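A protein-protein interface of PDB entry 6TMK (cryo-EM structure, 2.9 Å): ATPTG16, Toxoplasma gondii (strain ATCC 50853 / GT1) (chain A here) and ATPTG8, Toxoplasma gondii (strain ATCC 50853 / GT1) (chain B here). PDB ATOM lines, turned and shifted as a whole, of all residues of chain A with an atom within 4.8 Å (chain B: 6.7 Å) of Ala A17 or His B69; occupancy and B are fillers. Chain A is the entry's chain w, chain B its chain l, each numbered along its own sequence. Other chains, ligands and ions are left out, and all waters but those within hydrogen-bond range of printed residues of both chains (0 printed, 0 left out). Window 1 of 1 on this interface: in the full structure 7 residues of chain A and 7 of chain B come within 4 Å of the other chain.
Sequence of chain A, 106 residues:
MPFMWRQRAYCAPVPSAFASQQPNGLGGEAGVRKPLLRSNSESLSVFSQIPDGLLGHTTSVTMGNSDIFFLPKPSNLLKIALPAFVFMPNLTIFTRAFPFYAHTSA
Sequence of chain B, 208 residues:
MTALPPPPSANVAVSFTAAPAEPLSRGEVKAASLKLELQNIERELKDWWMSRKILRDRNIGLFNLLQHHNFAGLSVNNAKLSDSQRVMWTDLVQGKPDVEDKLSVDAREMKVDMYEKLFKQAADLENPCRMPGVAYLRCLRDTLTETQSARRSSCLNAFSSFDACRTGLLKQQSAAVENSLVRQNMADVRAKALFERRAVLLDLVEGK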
ATOM      1  N   PRO A  13     -22.676  26.529  33.834  1.00  0.00           N
ATOM      2  CA  PRO A  13     -23.332  25.765  32.776  1.00  0.00           C
ATOM      3  C   PRO A  13     -22.676  24.412  32.580  1.00  0.00           C
ATOM      4  O   PRO A  13     -21.526  24.174  32.955  1.00  0.00           O
ATOM      5  CB  PRO A  13     -23.172  26.648  31.535  1.00  0.00           C
ATOM      6  CG  PRO A  13     -22.109  27.572  31.841  1.00  0.00           C
ATOM      7  CD  PRO A  13     -22.002  27.724  33.308  1.00  0.00           C
ATOM      8  N   VAL A  14     -23.441  23.514  31.977  1.00  0.00           N
ATOM      9  CA  VAL A  14     -22.973  22.161  31.711  1.00  0.00           C
ATOM     10  C   VAL A  14     -21.994  22.202  30.545  1.00  0.00           C
ATOM     11  O   VAL A  14     -22.012  23.152  29.752  1.00  0.00           O
ATOM     12  CB  VAL A  14     -24.150  21.217  31.437  1.00  0.00           C
ATOM     13  CG1 VAL A  14     -25.117  21.263  32.587  1.00  0.00           C
ATOM     14  CG2 VAL A  14     -24.853  21.588  30.155  1.00  0.00           C
ATOM     15  N   PRO A  15     -21.117  21.210  30.411  1.00  0.00           N
ATOM     16  CA  PRO A  15     -20.143  21.237  29.312  1.00  0.00           C
ATOM     17  C   PRO A  15     -20.756  21.144  27.931  1.00  0.00           C
ATOM     18  O   PRO A  15     -20.081  21.487  26.953  1.00  0.00           O
ATOM     19  CB  PRO A  15     -19.245  20.030  29.614  1.00  0.00           C
ATOM     20  CG  PRO A  15     -19.969  19.232  30.612  1.00  0.00           C
ATOM     21  CD  PRO A  15     -20.801  20.163  31.390  1.00  0.00           C
ATOM     22  N   SER A  16     -22.000  20.687  27.806  1.00  0.00           N
ATOM     23  CA  SER A  16     -22.664  20.703  26.511  1.00  0.00           C
ATOM     24  C   SER A  16     -22.995  22.115  26.057  1.00  0.00           C
ATOM     25  O   SER A  16     -23.299  22.323  24.879  1.00  0.00           O
ATOM     26  CB  SER A  16     -23.938  19.863  26.568  1.00  0.00           C
ATOM     27  OG  SER A  16     -25.019  20.596  27.108  1.00  0.00           O
ATOM     28  N   ALA A  17     -22.941  23.086  26.966  1.00  0.00           N
ATOM     29  CA  ALA A  17     -23.268  24.463  26.635  1.00  0.00           C
ATOM     30  C   ALA A  17     -22.106  25.197  25.982  1.00  0.00           C
ATOM     31  O   ALA A  17     -22.329  26.096  25.168  1.00  0.00           O
ATOM     32  CB  ALA A  17     -23.708  25.197  27.894  1.00  0.00           C
ATOM     33  N   PHE A  18     -20.871  24.842  26.330  1.00  0.00           N
ATOM     34  CA  PHE A  18     -19.695  25.450  25.726  1.00  0.00           C
ATOM     35  C   PHE A  18     -19.423  24.963  24.311  1.00  0.00           C
ATOM     36  O   PHE A  18     -18.478  25.454  23.689  1.00  0.00           O
ATOM     37  CB  PHE A  18     -18.466  25.171  26.587  1.00  0.00           C
ATOM     38  CG  PHE A  18     -18.557  25.712  27.976  1.00  0.00           C
ATOM     39  CD1 PHE A  18     -18.092  26.972  28.273  1.00  0.00           C
ATOM     40  CD2 PHE A  18     -19.079  24.947  28.992  1.00  0.00           C
ATOM     41  CE1 PHE A  18     -18.168  27.462  29.548  1.00  0.00           C
ATOM     42  CE2 PHE A  18     -19.153  25.435  30.264  1.00  0.00           C
ATOM     43  CZ  PHE A  18     -18.697  26.691  30.544  1.00  0.00           C
ATOM     44  N   ALA A  19     -20.212  24.028  23.788  1.00  0.00           N
ATOM     45  CA  ALA A  19     -19.868  23.327  22.559  1.00  0.00           C
ATOM     46  C   ALA A  19     -20.323  24.027  21.287  1.00  0.00           C
ATOM     47  O   ALA A  19     -19.852  23.666  20.204  1.00  0.00           O
ATOM     48  CB  ALA A  19     -20.460  21.920  22.580  1.00  0.00           C
ATOM     49  N   SER A  20     -21.228  24.997  21.377  1.00  0.00           N
ATOM     50  CA  SER A  20     -21.649  25.794  20.227  1.00  0.00           C
ATOM     51  C   SER A  20     -22.339  24.958  19.157  1.00  0.00           C
ATOM     52  O   SER A  20     -22.469  25.397  18.012  1.00  0.00           O
ATOM     53  CB  SER A  20     -20.467  26.536  19.606  1.00  0.00           C
ATOM     54  OG  SER A  20     -20.902  27.408  18.584  1.00  0.00           O
ATOM     55  N   LEU A  36     -30.663  25.265  24.969  1.00  0.00           N
ATOM     56  CA  LEU A  36     -29.230  25.247  24.717  1.00  0.00           C
ATOM     57  C   LEU A  36     -28.414  25.443  25.982  1.00  0.00           C
ATOM     58  O   LEU A  36     -27.330  24.867  26.114  1.00  0.00           O
ATOM     59  CB  LEU A  36     -28.867  26.329  23.702  1.00  0.00           C
ATOM     60  CG  LEU A  36     -29.691  26.329  22.423  1.00  0.00           C
ATOM     61  CD1 LEU A  36     -29.332  27.519  21.586  1.00  0.00           C
ATOM     62  CD2 LEU A  36     -29.477  25.056  21.650  1.00  0.00           C
ATOM     63  N   LEU A  37     -28.917  26.249  26.906  1.00  0.00           N
ATOM     64  CA  LEU A  37     -28.229  26.586  28.142  1.00  0.00           C
ATOM     65  C   LEU A  37     -28.879  25.863  29.311  1.00  0.00           C
ATOM     66  O   LEU A  37     -30.092  25.962  29.510  1.00  0.00           O
ATOM     67  CB  LEU A  37     -28.260  28.095  28.361  1.00  0.00           C
ATOM     68  CG  LEU A  37     -27.368  28.705  29.428  1.00  0.00           C
ATOM     69  CD1 LEU A  37     -25.930  28.350  29.194  1.00  0.00           C
ATOM     70  CD2 LEU A  37     -27.544  30.199  29.377  1.00  0.00           C
ATOM     71  N   ASN B  64     -18.345  32.201  18.443  1.00  0.00           N
ATOM     72  CA  ASN B  64     -19.382  31.280  18.001  1.00  0.00           C
ATOM     73  C   ASN B  64     -20.274  30.862  19.158  1.00  0.00           C
ATOM     74  O   ASN B  64     -21.487  30.719  18.991  1.00  0.00           O
ATOM     75  CB  ASN B  64     -18.744  30.062  17.351  1.00  0.00           C
ATOM     76  CG  ASN B  64     -18.260  30.340  15.952  1.00  0.00           C
ATOM     77  OD1 ASN B  64     -18.850  31.131  15.218  1.00  0.00           O
ATOM     78  ND2 ASN B  64     -17.177  29.693  15.575  1.00  0.00           N
ATOM     79  N   LEU B  65     -19.698  30.694  20.344  1.00  0.00           N
ATOM     80  CA  LEU B  65     -20.492  30.353  21.516  1.00  0.00           C
ATOM     81  C   LEU B  65     -21.453  31.478  21.882  1.00  0.00           C
ATOM     82  O   LEU B  65     -22.625  31.231  22.196  1.00  0.00           O
ATOM     83  CB  LEU B  65     -19.557  30.048  22.677  1.00  0.00           C
ATOM     84  CG  LEU B  65     -20.163  29.715  24.028  1.00  0.00           C
ATOM     85  CD1 LEU B  65     -20.887  28.412  23.932  1.00  0.00           C
ATOM     86  CD2 LEU B  65     -19.087  29.655  25.073  1.00  0.00           C
ATOM     87  N   LEU B  66     -20.967  32.719  21.873  1.00  0.00           N
ATOM     88  CA  LEU B  66     -21.817  33.853  22.213  1.00  0.00           C
ATOM     89  C   LEU B  66     -22.902  34.065  21.166  1.00  0.00           C
ATOM     90  O   LEU B  66     -24.037  34.415  21.505  1.00  0.00           O
ATOM     91  CB  LEU B  66     -20.966  35.110  22.360  1.00  0.00           C
ATOM     92  CG  LEU B  66     -19.873  35.067  23.419  1.00  0.00           C
ATOM     93  CD1 LEU B  66     -18.838  36.126  23.136  1.00  0.00           C
ATOM     94  CD2 LEU B  66     -20.451  35.257  24.790  1.00  0.00           C
ATOM     95  N   GLN B  67     -22.573  33.854  19.893  1.00  0.00           N
ATOM     96  CA  GLN B  67     -23.579  33.920  18.843  1.00  0.00           C
ATOM     97  C   GLN B  67     -24.604  32.807  19.000  1.00  0.00           C
ATOM     98  O   GLN B  67     -25.788  33.002  18.706  1.00  0.00           O
ATOM     99  CB  GLN B  67     -22.894  33.848  17.481  1.00  0.00           C
ATOM    100  CG  GLN B  67     -23.547  34.655  16.393  1.00  0.00           C
ATOM    101  CD  GLN B  67     -22.904  34.426  15.047  1.00  0.00           C
ATOM    102  OE1 GLN B  67     -22.404  33.340  14.764  1.00  0.00           O
ATOM    103  NE2 GLN B  67     -22.914  35.450  14.204  1.00  0.00           N
ATOM    104  N   HIS B  68     -24.160  31.642  19.462  1.00  0.00           N
ATOM    105  CA  HIS B  68     -25.048  30.509  19.667  1.00  0.00           C
ATOM    106  C   HIS B  68     -26.035  30.784  20.789  1.00  0.00           C
ATOM    107  O   HIS B  68     -27.228  30.486  20.663  1.00  0.00           O
ATOM    108  CB  HIS B  68     -24.190  29.286  19.982  1.00  0.00           C
ATOM    109  CG  HIS B  68     -24.954  28.017  20.166  1.00  0.00           C
ATOM    110  ND1 HIS B  68     -24.813  27.232  21.288  1.00  0.00           N
ATOM    111  CD2 HIS B  68     -25.823  27.367  19.359  1.00  0.00           C
ATOM    112  CE1 HIS B  68     -25.584  26.167  21.176  1.00  0.00           C
ATOM    113  NE2 HIS B  68     -26.207  26.225  20.015  1.00  0.00           N
ATOM    114  N   HIS B  69     -25.553  31.332  21.897  1.00  0.00           N
ATOM    115  CA  HIS B  69     -26.398  31.667  23.033  1.00  0.00           C
ATOM    116  C   HIS B  69     -27.021  33.055  22.933  1.00  0.00           C
ATOM    117  O   HIS B  69     -27.672  33.496  23.884  1.00  0.00           O
ATOM    118  CB  HIS B  69     -25.594  31.538  24.321  1.00  0.00           C
ATOM    119  CG  HIS B  69     -25.266  30.125  24.676  1.00  0.00           C
ATOM    120  ND1 HIS B  69     -26.219  29.133  24.736  1.00  0.00           N
ATOM    121  CD2 HIS B  69     -24.085  29.529  24.957  1.00  0.00           C
ATOM    122  CE1 HIS B  69     -25.640  27.991  25.056  1.00  0.00           C
ATOM    123  NE2 HIS B  69     -24.347  28.204  25.195  1.00  0.00           N
ATOM    124  N   ASN B  70     -26.835  33.747  21.814  1.00  0.00           N
ATOM    125  CA  ASN B  70     -27.531  34.997  21.519  1.00  0.00           C
ATOM    126  C   ASN B  70     -27.226  36.071  22.567  1.00  0.00           C
ATOM    127  O   ASN B  70     -28.102  36.544  23.290  1.00  0.00           O
ATOM    128  CB  ASN B  70     -29.035  34.758  21.387  1.00  0.00           C
ATOM    129  CG  ASN B  70     -29.745  35.897  20.700  1.00  0.00           C
ATOM    130  OD1 ASN B  70     -29.139  36.673  19.966  1.00  0.00           O
ATOM    131  ND2 ASN B  70     -31.041  35.996  20.923  1.00  0.00           N
ATOM    132  N   PHE B  71     -25.957  36.451  22.630  1.00  0.00           N
ATOM    133  CA  PHE B  71     -25.490  37.490  23.532  1.00  0.00           C
ATOM    134  C   PHE B  71     -25.383  38.827  22.818  1.00  0.00           C
ATOM    135  O   PHE B  71     -25.209  38.897  21.599  1.00  0.00           O
ATOM    136  CB  PHE B  71     -24.136  37.138  24.144  1.00  0.00           C
ATOM    137  CG  PHE B  71     -24.224  36.299  25.374  1.00  0.00           C
ATOM    138  CD1 PHE B  71     -24.136  36.885  26.620  1.00  0.00           C
ATOM    139  CD2 PHE B  71     -24.404  34.939  25.296  1.00  0.00           C
ATOM    140  CE1 PHE B  71     -24.216  36.134  27.754  1.00  0.00           C
ATOM    141  CE2 PHE B  71     -24.487  34.181  26.434  1.00  0.00           C
ATOM    142  CZ  PHE B  71     -24.396  34.778  27.664  1.00  0.00           C
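The side-chain hydroxyl (OG) of Ser A20 lies within hydrogen-bond range of the backbone carbonyl oxygen (O) of Asn B64 (3.4 Å). O of Ala A17 lies within hydrogen-bond range of NE2 of His B69, 2.9 Å away.
Among the printed residues, pairs that only touch across the chains: Ala A17 with Leu B65 (3.0 Å), Phe A18 with Leu B65 (3.7 Å), Ser A20 with Leu B65 (3.9 Å), Ser A20 with His B68 (3.6 Å), Leu A36 with His B68 (3.7 Å) and Leu A36 with His B69 (3.7 Å).
Ala A17 touches just these residues of chain B: Leu B65 (3.0 Å) and His B69 (2.9 Å). Of the printed residues of chain B, Phe A18 touches Leu B65 (3.7 Å). Printed residues of chain A within 4 Å of Asn B64: Ser A20 (3.4 Å). Printed residues of chain A within 4 Å of His B68: Ser A20 and Leu A36. His B69 touches just these residues of chain A: Ala A17 (2.9 Å) and Leu A36 (3.7 Å). The nearest printed residue of chain B that does not touch Phe A18 is His B69 (5.0 Å).
Of the 8 printed residues of chain B, 4 touch a printed residue of chain A. Printed residues of chain B that touch a printed residue of chain A: Asn B64, Leu B65, His B68 and His B69. Hydrophobic or aromatic side chains of chain B within 4 Å of the printed part of chain A: Leu B65, His B68 and His B69. Of the 10 printed residues of chain A, 4 touch a printed residue of chain B. Printed residues of chain A that touch a printed residue of chain B: Ala A17, Phe A18, Ser A20 and Leu A36.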
